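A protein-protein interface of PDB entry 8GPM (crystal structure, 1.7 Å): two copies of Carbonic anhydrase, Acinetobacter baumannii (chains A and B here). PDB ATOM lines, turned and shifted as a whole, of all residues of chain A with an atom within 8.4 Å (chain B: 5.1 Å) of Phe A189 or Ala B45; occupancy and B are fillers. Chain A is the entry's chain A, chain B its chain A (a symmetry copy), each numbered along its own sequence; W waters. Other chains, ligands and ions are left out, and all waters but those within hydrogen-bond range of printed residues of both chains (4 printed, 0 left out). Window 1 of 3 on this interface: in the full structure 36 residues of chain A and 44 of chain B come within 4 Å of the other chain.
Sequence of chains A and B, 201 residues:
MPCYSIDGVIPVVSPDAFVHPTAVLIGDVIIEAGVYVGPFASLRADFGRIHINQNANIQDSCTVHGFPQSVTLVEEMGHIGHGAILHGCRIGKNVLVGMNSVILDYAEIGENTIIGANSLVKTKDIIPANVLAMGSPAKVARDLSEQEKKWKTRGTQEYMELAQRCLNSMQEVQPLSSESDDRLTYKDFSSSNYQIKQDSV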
ATOM      1  N   ASP A  60     -15.981  37.063  10.220  1.00  0.00           N
ATOM      2  CA  ASP A  60     -16.489  36.731  11.552  1.00  0.00           C
ATOM      3  C   ASP A  60     -16.321  37.917  12.507  1.00  0.00           C
ATOM      4  O   ASP A  60     -15.262  38.567  12.550  1.00  0.00           O
ATOM      5  CB  ASP A  60     -15.747  35.560  12.195  1.00  0.00           C
ATOM      6  CG  ASP A  60     -15.418  34.444  11.215  1.00  0.00           C
ATOM      7  OD1 ASP A  60     -14.742  34.771  10.217  1.00  0.00           O
ATOM      8  OD2 ASP A  60     -15.946  33.304  11.385  1.00  0.00           O
ATOM      9  N   LEU A 162     -17.691  29.648  -1.119  1.00  0.00           N
ATOM     10  CA  LEU A 162     -18.101  29.330   0.250  1.00  0.00           C
ATOM     11  C   LEU A 162     -19.591  29.612   0.472  1.00  0.00           C
ATOM     12  O   LEU A 162     -20.298  28.822   1.107  1.00  0.00           O
ATOM     13  CB  LEU A 162     -17.258  30.141   1.257  1.00  0.00           C
ATOM     14  CG  LEU A 162     -17.576  29.882   2.741  1.00  0.00           C
ATOM     15  CD1 LEU A 162     -17.293  28.399   3.081  1.00  0.00           C
ATOM     16  CD2 LEU A 162     -16.812  30.842   3.698  1.00  0.00           C
ATOM     17  N   ARG A 165     -21.445  26.711  -0.937  1.00  0.00           N
ATOM     18  CA  ARG A 165     -21.263  25.502  -0.126  1.00  0.00           C
ATOM     19  C   ARG A 165     -22.114  25.581   1.124  1.00  0.00           C
ATOM     20  O   ARG A 165     -22.667  24.576   1.572  1.00  0.00           O
ATOM     21  CB  ARG A 165     -19.783  25.322   0.297  1.00  0.00           C
ATOM     22  CG  ARG A 165     -18.805  24.936  -0.806  1.00  0.00           C
ATOM     23  CD  ARG A 165     -17.366  25.131  -0.321  1.00  0.00           C
ATOM     24  NE  ARG A 165     -16.992  24.208   0.758  1.00  0.00           N
ATOM     25  CZ  ARG A 165     -16.052  24.472   1.661  1.00  0.00           C
ATOM     26  NH1 ARG A 165     -15.388  25.626   1.653  1.00  0.00           N
ATOM     27  NH2 ARG A 165     -15.759  23.554   2.595  1.00  0.00           N
ATOM     28  N   SER A 169     -24.946  23.050   2.121  1.00  0.00           N
ATOM     29  CA  SER A 169     -24.714  21.975   3.081  1.00  0.00           C
ATOM     30  C   SER A 169     -24.454  22.394   4.516  1.00  0.00           C
ATOM     31  O   SER A 169     -24.174  21.512   5.331  1.00  0.00           O
ATOM     32  CB  SER A 169     -23.533  21.114   2.572  1.00  0.00           C
ATOM     33  OG  SER A 169     -22.283  21.759   2.791  1.00  0.00           O
ATOM     34  N   MET A 170     -24.514  23.667   4.893  1.00  0.00           N
ATOM     35  CA  MET A 170     -24.176  23.917   6.280  1.00  0.00           C
ATOM     36  C   MET A 170     -25.414  23.622   7.130  1.00  0.00           C
ATOM     37  O   MET A 170     -26.541  24.009   6.777  1.00  0.00           O
ATOM     38  CB  MET A 170     -23.636  25.331   6.481  1.00  0.00           C
ATOM     39  CG  MET A 170     -23.738  25.836   7.941  1.00  0.00           C
ATOM     40  SD  MET A 170     -22.537  27.144   8.158  1.00  0.00           S
ATOM     41  CE  MET A 170     -21.004  26.430   7.574  1.00  0.00           C
ATOM     42  N   ARG A 183     -14.101   9.339   9.662  1.00  0.00           N
ATOM     43  CA  ARG A 183     -14.817  10.604   9.593  1.00  0.00           C
ATOM     44  C   ARG A 183     -14.319  11.429   8.409  1.00  0.00           C
ATOM     45  O   ARG A 183     -13.161  11.323   7.994  1.00  0.00           O
ATOM     46  CB  ARG A 183     -14.692  11.399  10.906  1.00  0.00           C
ATOM     47  CG  ARG A 183     -13.344  11.989  11.223  1.00  0.00           C
ATOM     48  CD  ARG A 183     -13.478  12.937  12.478  1.00  0.00           C
ATOM     49  NE  ARG A 183     -14.084  14.237  12.185  1.00  0.00           N
ATOM     50  CZ  ARG A 183     -13.365  15.340  11.984  1.00  0.00           C
ATOM     51  NH1 ARG A 183     -12.042  15.309  12.027  1.00  0.00           N
ATOM     52  NH2 ARG A 183     -13.989  16.511  11.773  1.00  0.00           N
ATOM     53  N   LEU A 184     -15.221  12.220   7.844  1.00  0.00           N
ATOM     54  CA  LEU A 184     -14.852  13.238   6.866  1.00  0.00           C
ATOM     55  C   LEU A 184     -14.020  14.339   7.534  1.00  0.00           C
ATOM     56  O   LEU A 184     -14.262  14.702   8.688  1.00  0.00           O
ATOM     57  CB  LEU A 184     -16.135  13.831   6.270  1.00  0.00           C
ATOM     58  CG  LEU A 184     -17.035  12.840   5.516  1.00  0.00           C
ATOM     59  CD1 LEU A 184     -18.172  13.567   4.810  1.00  0.00           C
ATOM     60  CD2 LEU A 184     -16.222  12.052   4.519  1.00  0.00           C
ATOM     61  N   THR A 185     -13.043  14.878   6.799  1.00  0.00           N
ATOM     62  CA  THR A 185     -12.133  15.889   7.347  1.00  0.00           C
ATOM     63  C   THR A 185     -11.972  17.011   6.332  1.00  0.00           C
ATOM     64  O   THR A 185     -12.590  17.000   5.263  1.00  0.00           O
ATOM     65  CB  THR A 185     -10.746  15.319   7.649  1.00  0.00           C
ATOM     66  OG1 THR A 185     -10.142  14.961   6.402  1.00  0.00           O
ATOM     67  CG2 THR A 185     -10.790  14.069   8.575  1.00  0.00           C
ATOM     68  N   TYR A 186     -11.110  17.990   6.664  1.00  0.00           N
ATOM     69  CA  TYR A 186     -10.835  19.051   5.706  1.00  0.00           C
ATOM     70  C   TYR A 186     -10.279  18.503   4.388  1.00  0.00           C
ATOM     71  O   TYR A 186     -10.372  19.182   3.364  1.00  0.00           O
ATOM     72  CB  TYR A 186      -9.883  20.093   6.312  1.00  0.00           C
ATOM     73  CG  TYR A 186      -8.416  19.693   6.383  1.00  0.00           C
ATOM     74  CD1 TYR A 186      -7.986  18.649   7.214  1.00  0.00           C
ATOM     75  CD2 TYR A 186      -7.457  20.375   5.621  1.00  0.00           C
ATOM     76  CE1 TYR A 186      -6.626  18.316   7.299  1.00  0.00           C
ATOM     77  CE2 TYR A 186      -6.122  20.060   5.698  1.00  0.00           C
ATOM     78  CZ  TYR A 186      -5.710  19.033   6.515  1.00  0.00           C
ATOM     79  OH  TYR A 186      -4.376  18.730   6.599  1.00  0.00           O
ATOM     80  N   LYS A 187      -9.741  17.280   4.374  1.00  0.00           N
ATOM     81  CA  LYS A 187      -9.234  16.729   3.126  1.00  0.00           C
ATOM     82  C   LYS A 187     -10.362  16.391   2.162  1.00  0.00           C
ATOM     83  O   LYS A 187     -10.107  16.186   0.971  1.00  0.00           O
ATOM     84  CB  LYS A 187      -8.389  15.493   3.421  1.00  0.00           C
ATOM     85  CG  LYS A 187      -7.020  15.790   4.094  1.00  0.00           C
ATOM     86  CD  LYS A 187      -6.338  17.040   3.567  1.00  0.00           C
ATOM     87  CE  LYS A 187      -5.626  16.732   2.250  1.00  0.00           C
ATOM     88  NZ  LYS A 187      -4.795  17.861   1.699  1.00  0.00           N
ATOM     89  N   ASP A 188     -11.595  16.340   2.650  1.00  0.00           N
ATOM     90  CA  ASP A 188     -12.745  16.077   1.808  1.00  0.00           C
ATOM     91  C   ASP A 188     -13.375  17.348   1.263  1.00  0.00           C
ATOM     92  O   ASP A 188     -14.348  17.250   0.513  1.00  0.00           O
ATOM     93  CB  ASP A 188     -13.758  15.237   2.576  1.00  0.00           C
ATOM     94  CG  ASP A 188     -13.177  13.893   2.981  1.00  0.00           C
ATOM     95  OD1 ASP A 188     -12.939  13.060   2.098  1.00  0.00           O
ATOM     96  OD2 ASP A 188     -12.946  13.662   4.185  1.00  0.00           O
ATOM     97  N   PHE A 189     -12.869  18.528   1.637  1.00  0.00           N
ATOM     98  CA  PHE A 189     -13.269  19.765   0.968  1.00  0.00           C
ATOM     99  C   PHE A 189     -12.718  19.781  -0.468  1.00  0.00           C
ATOM    100  O   PHE A 189     -11.575  19.367  -0.724  1.00  0.00           O
ATOM    101  CB  PHE A 189     -12.718  21.005   1.695  1.00  0.00           C
ATOM    102  CG  PHE A 189     -13.235  21.201   3.117  1.00  0.00           C
ATOM    103  CD1 PHE A 189     -14.438  20.633   3.544  1.00  0.00           C
ATOM    104  CD2 PHE A 189     -12.475  21.934   4.033  1.00  0.00           C
ATOM    105  CE1 PHE A 189     -14.907  20.827   4.846  1.00  0.00           C
ATOM    106  CE2 PHE A 189     -12.924  22.122   5.353  1.00  0.00           C
ATOM    107  CZ  PHE A 189     -14.161  21.567   5.759  1.00  0.00           C
ATOM    108  N   SER A 190     -13.512  20.348  -1.389  1.00  0.00           N
ATOM    109  CA  SER A 190     -13.118  20.487  -2.800  1.00  0.00           C
ATOM    110  C   SER A 190     -11.738  21.130  -2.972  1.00  0.00           C
ATOM    111  O   SER A 190     -11.004  20.802  -3.913  1.00  0.00           O
ATOM    112  CB  SER A 190     -14.165  21.321  -3.545  1.00  0.00           C
ATOM    113  OG  SER A 190     -15.460  20.782  -3.369  1.00  0.00           O
ATOM    114  N   SER A 191     -11.386  22.078  -2.096  1.00  0.00           N
ATOM    115  CA  SER A 191     -10.071  22.721  -2.132  1.00  0.00           C
ATOM    116  C   SER A 191      -8.919  21.721  -2.118  1.00  0.00           C
ATOM    117  O   SER A 191      -7.783  22.087  -2.460  1.00  0.00           O
ATOM    118  CB  SER A 191      -9.918  23.668  -0.937  1.00  0.00           C
ATOM    119  N   SER A 192      -9.176  20.475  -1.698  1.00  0.00           N
ATOM    120  CA  SER A 192      -8.125  19.466  -1.661  1.00  0.00           C
ATOM    121  C   SER A 192      -7.677  19.079  -3.067  1.00  0.00           C
ATOM    122  O   SER A 192      -6.536  18.635  -3.251  1.00  0.00           O
ATOM    123  CB  SER A 192      -8.615  18.236  -0.884  1.00  0.00           C
ATOM    124  OG  SER A 192      -7.648  17.205  -0.868  1.00  0.00           O
ATOM    125  N   ASN A 193      -8.548  19.247  -4.063  1.00  0.00           N
ATOM    126  CA  ASN A 193      -8.241  18.915  -5.456  1.00  0.00           C
ATOM    127  C   ASN A 193      -7.699  20.125  -6.230  1.00  0.00           C
ATOM    128  O   ASN A 193      -7.601  21.237  -5.695  1.00  0.00           O
ATOM    129  CB  ASN A 193      -9.489  18.363  -6.155  1.00  0.00           C
ATOM    130  N   ILE B   6     -20.108  21.267   7.416  1.00  0.00           N
ATOM    131  CA  ILE B   6     -20.066  21.786   6.052  1.00  0.00           C
ATOM    132  C   ILE B   6     -19.457  20.695   5.207  1.00  0.00           C
ATOM    133  O   ILE B   6     -18.495  20.054   5.635  1.00  0.00           O
ATOM    134  CB  ILE B   6     -19.279  23.114   5.952  1.00  0.00           C
ATOM    135  CG1 ILE B   6     -19.438  23.714   4.530  1.00  0.00           C
ATOM    136  CG2 ILE B   6     -17.818  22.908   6.324  1.00  0.00           C
ATOM    137  CD1 ILE B   6     -18.690  25.058   4.330  1.00  0.00           C
ATOM    138  N   ASP B   7     -20.070  20.413   4.056  1.00  0.00           N
ATOM    139  CA  ASP B   7     -19.627  19.314   3.199  1.00  0.00           C
ATOM    140  C   ASP B   7     -19.584  17.996   3.970  1.00  0.00           C
ATOM    141  O   ASP B   7     -18.807  17.093   3.622  1.00  0.00           O
ATOM    142  CB  ASP B   7     -18.245  19.597   2.596  1.00  0.00           C
ATOM    143  CG  ASP B   7     -18.275  20.683   1.541  1.00  0.00           C
ATOM    144  OD1 ASP B   7     -19.247  20.737   0.780  1.00  0.00           O
ATOM    145  OD2 ASP B   7     -17.334  21.506   1.498  1.00  0.00           O
ATOM    146  N   VAL B   9     -18.591  17.506   7.025  1.00  0.00           N
ATOM    147  CA  VAL B   9     -17.497  17.447   7.998  1.00  0.00           C
ATOM    148  C   VAL B   9     -17.988  18.014   9.320  1.00  0.00           C
ATOM    149  O   VAL B   9     -18.484  19.157   9.375  1.00  0.00           O
ATOM    150  CB  VAL B   9     -16.270  18.219   7.479  1.00  0.00           C
ATOM    151  CG1 VAL B   9     -15.141  18.191   8.516  1.00  0.00           C
ATOM    152  CG2 VAL B   9     -15.800  17.671   6.129  1.00  0.00           C
ATOM    153  N   ILE B  26     -17.361  25.296  13.162  1.00  0.00           N
ATOM    154  CA  ILE B  26     -17.773  24.925  11.801  1.00  0.00           C
ATOM    155  C   ILE B  26     -16.761  23.951  11.214  1.00  0.00           C
ATOM    156  O   ILE B  26     -15.561  24.246  11.190  1.00  0.00           O
ATOM    157  CB  ILE B  26     -17.898  26.148  10.874  1.00  0.00           C
ATOM    158  CG1 ILE B  26     -19.180  26.915  11.206  1.00  0.00           C
ATOM    159  CG2 ILE B  26     -17.931  25.669   9.416  1.00  0.00           C
ATOM    160  CD1 ILE B  26     -19.106  28.399  10.698  1.00  0.00           C
ATOM    161  N   GLY B  27     -17.251  22.821  10.702  1.00  0.00           N
ATOM    162  CA  GLY B  27     -16.378  21.972   9.878  1.00  0.00           C
ATOM    163  C   GLY B  27     -15.324  21.200  10.662  1.00  0.00           C
ATOM    164  O   GLY B  27     -15.630  20.604  11.708  1.00  0.00           O
ATOM    165  N   ASP B  28     -14.076  21.198  10.187  1.00  0.00           N
ATOM    166  CA  ASP B  28     -13.065  20.298  10.762  1.00  0.00           C
ATOM    167  C   ASP B  28     -12.328  20.975  11.921  1.00  0.00           C
ATOM    168  O   ASP B  28     -11.130  21.277  11.850  1.00  0.00           O
ATOM    169  CB  ASP B  28     -12.079  19.839   9.686  1.00  0.00           C
ATOM    170  CG  ASP B  28     -11.259  18.624  10.129  1.00  0.00           C
ATOM    171  OD1 ASP B  28     -11.584  18.061  11.203  1.00  0.00           O
ATOM    172  OD2 ASP B  28     -10.309  18.213   9.409  1.00  0.00           O
ATOM    173  N   VAL B  29     -13.074  21.177  13.008  1.00  0.00           N
ATOM    174  CA  VAL B  29     -12.544  21.670  14.283  1.00  0.00           C
ATOM    175  C   VAL B  29     -12.447  20.501  15.247  1.00  0.00           C
ATOM    176  O   VAL B  29     -13.417  19.758  15.417  1.00  0.00           O
ATOM    177  CB  VAL B  29     -13.466  22.727  14.918  1.00  0.00           C
ATOM    178  CG1 VAL B  29     -12.834  23.167  16.270  1.00  0.00           C
ATOM    179  CG2 VAL B  29     -13.711  23.877  14.013  1.00  0.00           C
ATOM    180  N   LEU B  43     -14.675  29.305  15.663  1.00  0.00           N
ATOM    181  CA  LEU B  43     -13.663  28.331  15.233  1.00  0.00           C
ATOM    182  C   LEU B  43     -14.125  27.797  13.885  1.00  0.00           C
ATOM    183  O   LEU B  43     -14.931  26.851  13.820  1.00  0.00           O
ATOM    184  CB  LEU B  43     -13.510  27.197  16.245  1.00  0.00           C
ATOM    185  CG  LEU B  43     -13.191  27.740  17.640  1.00  0.00           C
ATOM    186  CD1 LEU B  43     -12.936  26.598  18.667  1.00  0.00           C
ATOM    187  CD2 LEU B  43     -11.987  28.641  17.563  1.00  0.00           C
ATOM    188  N   ARG B  44     -13.667  28.431  12.796  1.00  0.00           N
ATOM    189  CA  ARG B  44     -14.290  28.215  11.473  1.00  0.00           C
ATOM    190  C   ARG B  44     -13.341  27.391  10.622  1.00  0.00           C
ATOM    191  O   ARG B  44     -12.393  27.918  10.028  1.00  0.00           O
ATOM    192  CB  ARG B  44     -14.671  29.556  10.806  1.00  0.00           C
ATOM    193  CG  ARG B  44     -15.444  29.349   9.475  1.00  0.00           C
ATOM    194  CD  ARG B  44     -16.367  30.550   9.190  1.00  0.00           C
ATOM    195  NE  ARG B  44     -15.643  31.813   8.965  1.00  0.00           N
ATOM    196  CZ  ARG B  44     -15.269  32.280   7.779  1.00  0.00           C
ATOM    197  NH1 ARG B  44     -15.312  31.517   6.674  1.00  0.00           N
ATOM    198  NH2 ARG B  44     -14.805  33.534   7.693  1.00  0.00           N
ATOM    199  N   ALA B  45     -13.582  26.074  10.573  1.00  0.00           N
ATOM    200  CA  ALA B  45     -12.724  25.158   9.821  1.00  0.00           C
ATOM    201  C   ALA B  45     -13.453  24.740   8.535  1.00  0.00           C
ATOM    202  O   ALA B  45     -13.755  23.558   8.301  1.00  0.00           O
ATOM    203  CB  ALA B  45     -12.325  23.961  10.712  1.00  0.00           C
ATOM    204  N   ASP B  46     -13.788  25.735   7.694  1.00  0.00           N
ATOM    205  CA  ASP B  46     -14.440  25.516   6.409  1.00  0.00           C
ATOM    206  C   ASP B  46     -13.496  25.606   5.230  1.00  0.00           C
ATOM    207  O   ASP B  46     -13.881  25.211   4.117  1.00  0.00           O
ATOM    208  CB  ASP B  46     -15.606  26.523   6.231  1.00  0.00           C
ATOM    209  CG  ASP B  46     -15.170  27.991   6.354  1.00  0.00           C
ATOM    210  OD1 ASP B  46     -13.955  28.271   6.460  1.00  0.00           O
ATOM    211  OD2 ASP B  46     -16.073  28.864   6.329  1.00  0.00           O
ATOM    212  N   PHE B  47     -12.265  26.088   5.448  1.00  0.00           N
ATOM    213  CA  PHE B  47     -11.233  25.996   4.432  1.00  0.00           C
ATOM    214  C   PHE B  47     -10.165  24.971   4.786  1.00  0.00           C
ATOM    215  O   PHE B  47      -9.637  24.276   3.902  1.00  0.00           O
ATOM    216  CB  PHE B  47     -10.548  27.368   4.227  1.00  0.00           C
ATOM    217  CG  PHE B  47     -11.428  28.430   3.559  1.00  0.00           C
ATOM    218  CD1 PHE B  47     -12.629  28.101   2.968  1.00  0.00           C
ATOM    219  CD2 PHE B  47     -11.013  29.745   3.515  1.00  0.00           C
ATOM    220  CE1 PHE B  47     -13.415  29.074   2.348  1.00  0.00           C
ATOM    221  CE2 PHE B  47     -11.789  30.725   2.911  1.00  0.00           C
ATOM    222  CZ  PHE B  47     -12.997  30.391   2.344  1.00  0.00           C
ATOM    223  N   GLY B  48      -9.814  24.889   6.055  1.00  0.00           N
ATOM    224  CA  GLY B  48      -8.820  23.931   6.529  1.00  0.00           C
ATOM    225  C   GLY B  48      -9.222  23.337   7.864  1.00  0.00           C
ATOM    226  O   GLY B  48     -10.398  23.382   8.227  1.00  0.00           O
ATOM    227  N   ARG B  49      -8.253  22.817   8.619  1.00  0.00           N
ATOM    228  CA  ARG B  49      -8.510  22.197   9.908  1.00  0.00           C
ATOM    229  C   ARG B  49      -8.120  23.149  11.039  1.00  0.00           C
ATOM    230  O   ARG B  49      -7.197  23.946  10.902  1.00  0.00           O
ATOM    231  CB  ARG B  49      -7.692  20.910  10.020  1.00  0.00           C
ATOM    232  CG  ARG B  49      -7.532  20.409  11.438  1.00  0.00           C
ATOM    233  CD  ARG B  49      -6.986  19.010  11.516  1.00  0.00           C
ATOM    234  NE  ARG B  49      -7.894  18.041  10.930  1.00  0.00           N
ATOM    235  CZ  ARG B  49      -7.821  16.733  11.093  1.00  0.00           C
ATOM    236  NH1 ARG B  49      -6.855  16.166  11.810  1.00  0.00           N
ATOM    237  NH2 ARG B  49      -8.753  15.966  10.545  1.00  0.00           N
ATOM    238  N   ILE B  50      -8.784  23.011  12.180  1.00  0.00           N
ATOM    239  CA  ILE B  50      -8.389  23.701  13.409  1.00  0.00           C
ATOM    240  C   ILE B  50      -8.273  22.631  14.462  1.00  0.00           C
ATOM    241  O   ILE B  50      -9.178  21.800  14.593  1.00  0.00           O
ATOM    242  CB  ILE B  50      -9.436  24.769  13.835  1.00  0.00           C
ATOM    243  CG1 ILE B  50      -9.491  25.881  12.782  1.00  0.00           C
ATOM    244  CG2 ILE B  50      -9.190  25.286  15.292  1.00  0.00           C
ATOM    245  CD1 ILE B  50     -10.762  26.821  12.974  1.00  0.00           C
ATOM    246  N   GLN B  69      -6.941  24.320   2.884  1.00  0.00           N
ATOM    247  CA  GLN B  69      -6.069  23.196   3.211  1.00  0.00           C
ATOM    248  C   GLN B  69      -5.005  23.548   4.250  1.00  0.00           C
ATOM    249  O   GLN B  69      -4.045  22.798   4.442  1.00  0.00           O
ATOM    250  CB  GLN B  69      -5.439  22.623   1.931  1.00  0.00           C
ATOM    251  CG  GLN B  69      -6.423  21.899   0.985  1.00  0.00           C
ATOM    252  CD  GLN B  69      -7.317  20.887   1.694  1.00  0.00           C
ATOM    253  OE1 GLN B  69      -6.848  19.803   2.010  1.00  0.00           O
ATOM    254  NE2 GLN B  69      -8.608  21.176   1.829  1.00  0.00           N
HETATM  255  O   HOH W   1      -9.965  13.317  12.233  1.00  0.00           O
HETATM  256  O   HOH W   2     -21.308  21.898  -0.114  1.00  0.00           O
HETATM  257  O   HOH W   3     -17.421  16.009   1.586  1.00  0.00           O
HETATM  258  O   HOH W   4     -15.537  21.715  -0.804  1.00  0.00           O
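The guanidinium group (NH2) of Arg B44 is in salt-bridge range of the side-chain carboxylate (OD1) of Asp A60, 2.8 Å away.
The side-chain carboxylate of Asp B7 lies within salt-bridge range of the guanidinium group of Arg A165 (2.8 Å).
The guanidinium group of Arg A165 is in hydrogen-bond range of the backbone carbonyl oxygen of Asp B46 (2.9 Å).
OG of Ser A169 is in hydrogen-bond range of N of Asp B7 (2.9 Å).
The guanidinium group (NH1) of Arg A183 is in salt-bridge range of the side-chain carboxylate (OD1) of Asp B28, 2.9 Å away.
N of Tyr A186 lies within hydrogen-bond range of OD2 of Asp B28 (2.9 Å).
The backbone carbonyl oxygen (O) of Tyr A186 is in hydrogen-bond range of the side-chain amide nitrogen (NE2) of Gln B69 (3.1 Å).
OE1 of Gln B69 sits at hydrogen-bond distance from NZ of Lys A187 (2.8 Å).
OG of Ser A169 is in hydrogen-bond range of O of Arg A165 (3.1 Å).
The side-chain hydroxyl (OG1) of Thr A185 lies close to the backbone NH (N) of Lys A187 (3.1 Å).
N of Thr A185 sits at hydrogen-bond distance from OD2 of Asp A188 (2.9 Å).
The backbone carbonyl oxygen of Lys A187 sits close to the side-chain hydroxyl of Ser A192 (3.2 Å).
The backbone carbonyl oxygen (O) of Ile B26 sits at hydrogen-bond distance from the backbone NH (N) of Ala B45 (2.8 Å).
OD2 of Asp B28 is in salt-bridge range of NE of Arg B49.
Among the printed residues, merely in contact across the chains: Leu A162 with Ile B6 (3.8 Å), Leu A162 with Arg B44 (3.4 Å), Leu A162 with Asp B46 (3.4 Å), Arg A165 with Ile B6 (3.7 Å), Arg A165 with Phe B47 (3.9 Å), Ser A169 with Ile B6 (3.9 Å), Met A170 with Ile B26 (3.7 Å), Arg A183 with Val B9 (3.8 Å), Arg A183 with Arg B49 (3.7 Å), Leu A184 with Asp B7 (3.8 Å), Leu A184 with Val B9 (3.6 Å), Thr A185 with Val B9 (3.4 Å), Thr A185 with Asp B28 (3.4 Å), Thr A185 with Arg B49 (3.4 Å), Tyr A186 with Gly B48 (3.7 Å), Tyr A186 with Arg B49 (3.6 Å), Phe A189 with Ile B6 (3.8 Å), Phe A189 with Asp B7 (3.7 Å), Phe A189 with Val B9 (3.5 Å), Phe A189 with Ala B45 (3.3 Å), Phe A189 with Asp B46 (3.5 Å), Phe A189 with Phe B47 (3.7 Å), Ser A191 with Gln B69 (3.7 Å) and Ser A192 with Gln B69 (3.6 Å).
Asp A188 touches none of the printed residues of chain B.
Phe A189 touches just these residues of chain B: Ile B6, Asp B7, Val B9, Ala B45, Asp B46 and Phe B47.
Of the printed residues of chain A, Arg B44 touches Asp A60 (2.8 Å) and Leu A162 (3.4 Å).
Ala B45 touches just one residue of chain A: Phe A189 (3.3 Å).
Of the printed residues of chain A, Phe B47 touches Arg A165 and Phe A189.
Printed residues of chain A within 4 Å of Gln B69: Tyr A186, Lys A187, Ser A191 and Ser A192.
The nearest residue of chain A that does not touch Ala B45 is Tyr A186 (5.6 Å).
The nearest printed residue of chain B that does not touch Ser A191 is Phe B47 (4.9 Å).
Printed residues of chain A that touch a printed residue of chain B: Asp A60, Leu A162, Arg A165, Ser A169, Met A170, Arg A183, Leu A184, Thr A185, Tyr A186, Lys A187, Phe A189, Ser A191 and Ser A192.
Of the 16 printed residues of chain B, 12 touch a printed residue of chain A.
Hydrophobic or aromatic side chains of chain B within 4 Å of the printed part of chain A: Ile B6, Val B9, Ile B26 and Phe B47.
Among the printed residues, Asp or Glu carboxylates within 4 Å of a Lys or Arg side-chain nitrogen of the other chain: Asp A60 with Arg B44 (2.8 Å), Arg A165 with Asp B7 (2.8 Å) and Arg A183 with Asp B28 (2.9 Å).
No position is printed for both chains.
Of the 32 pairs that touch across the chains among the printed residues, none has its exchanged pair printed and touching as well.
Water W4 lies within hydrogen-bond range of the backbone NH of Ser A190 (2.5 Å), the side-chain carboxylate of Asp B7 (2.9 Å) and the guanidinium group of Arg A165 (3.3 Å).
Water W2 lies within hydrogen-bond range of the side-chain carboxylate (OD1) of Asp B7 (2.5 Å), the side-chain hydroxyl (OG) of Ser A169 (3.1 Å) and the backbone carbonyl oxygen (O) of Arg A165 (3.4 Å).
Water W3 bridges O of Asp B7 (2.7 Å) and O of Asp A188 (3.5 Å).
Water W1 lies within hydrogen-bond range of NH1 of Arg A183 (2.9 Å) and NH2 of Arg B49 (3.4 Å).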
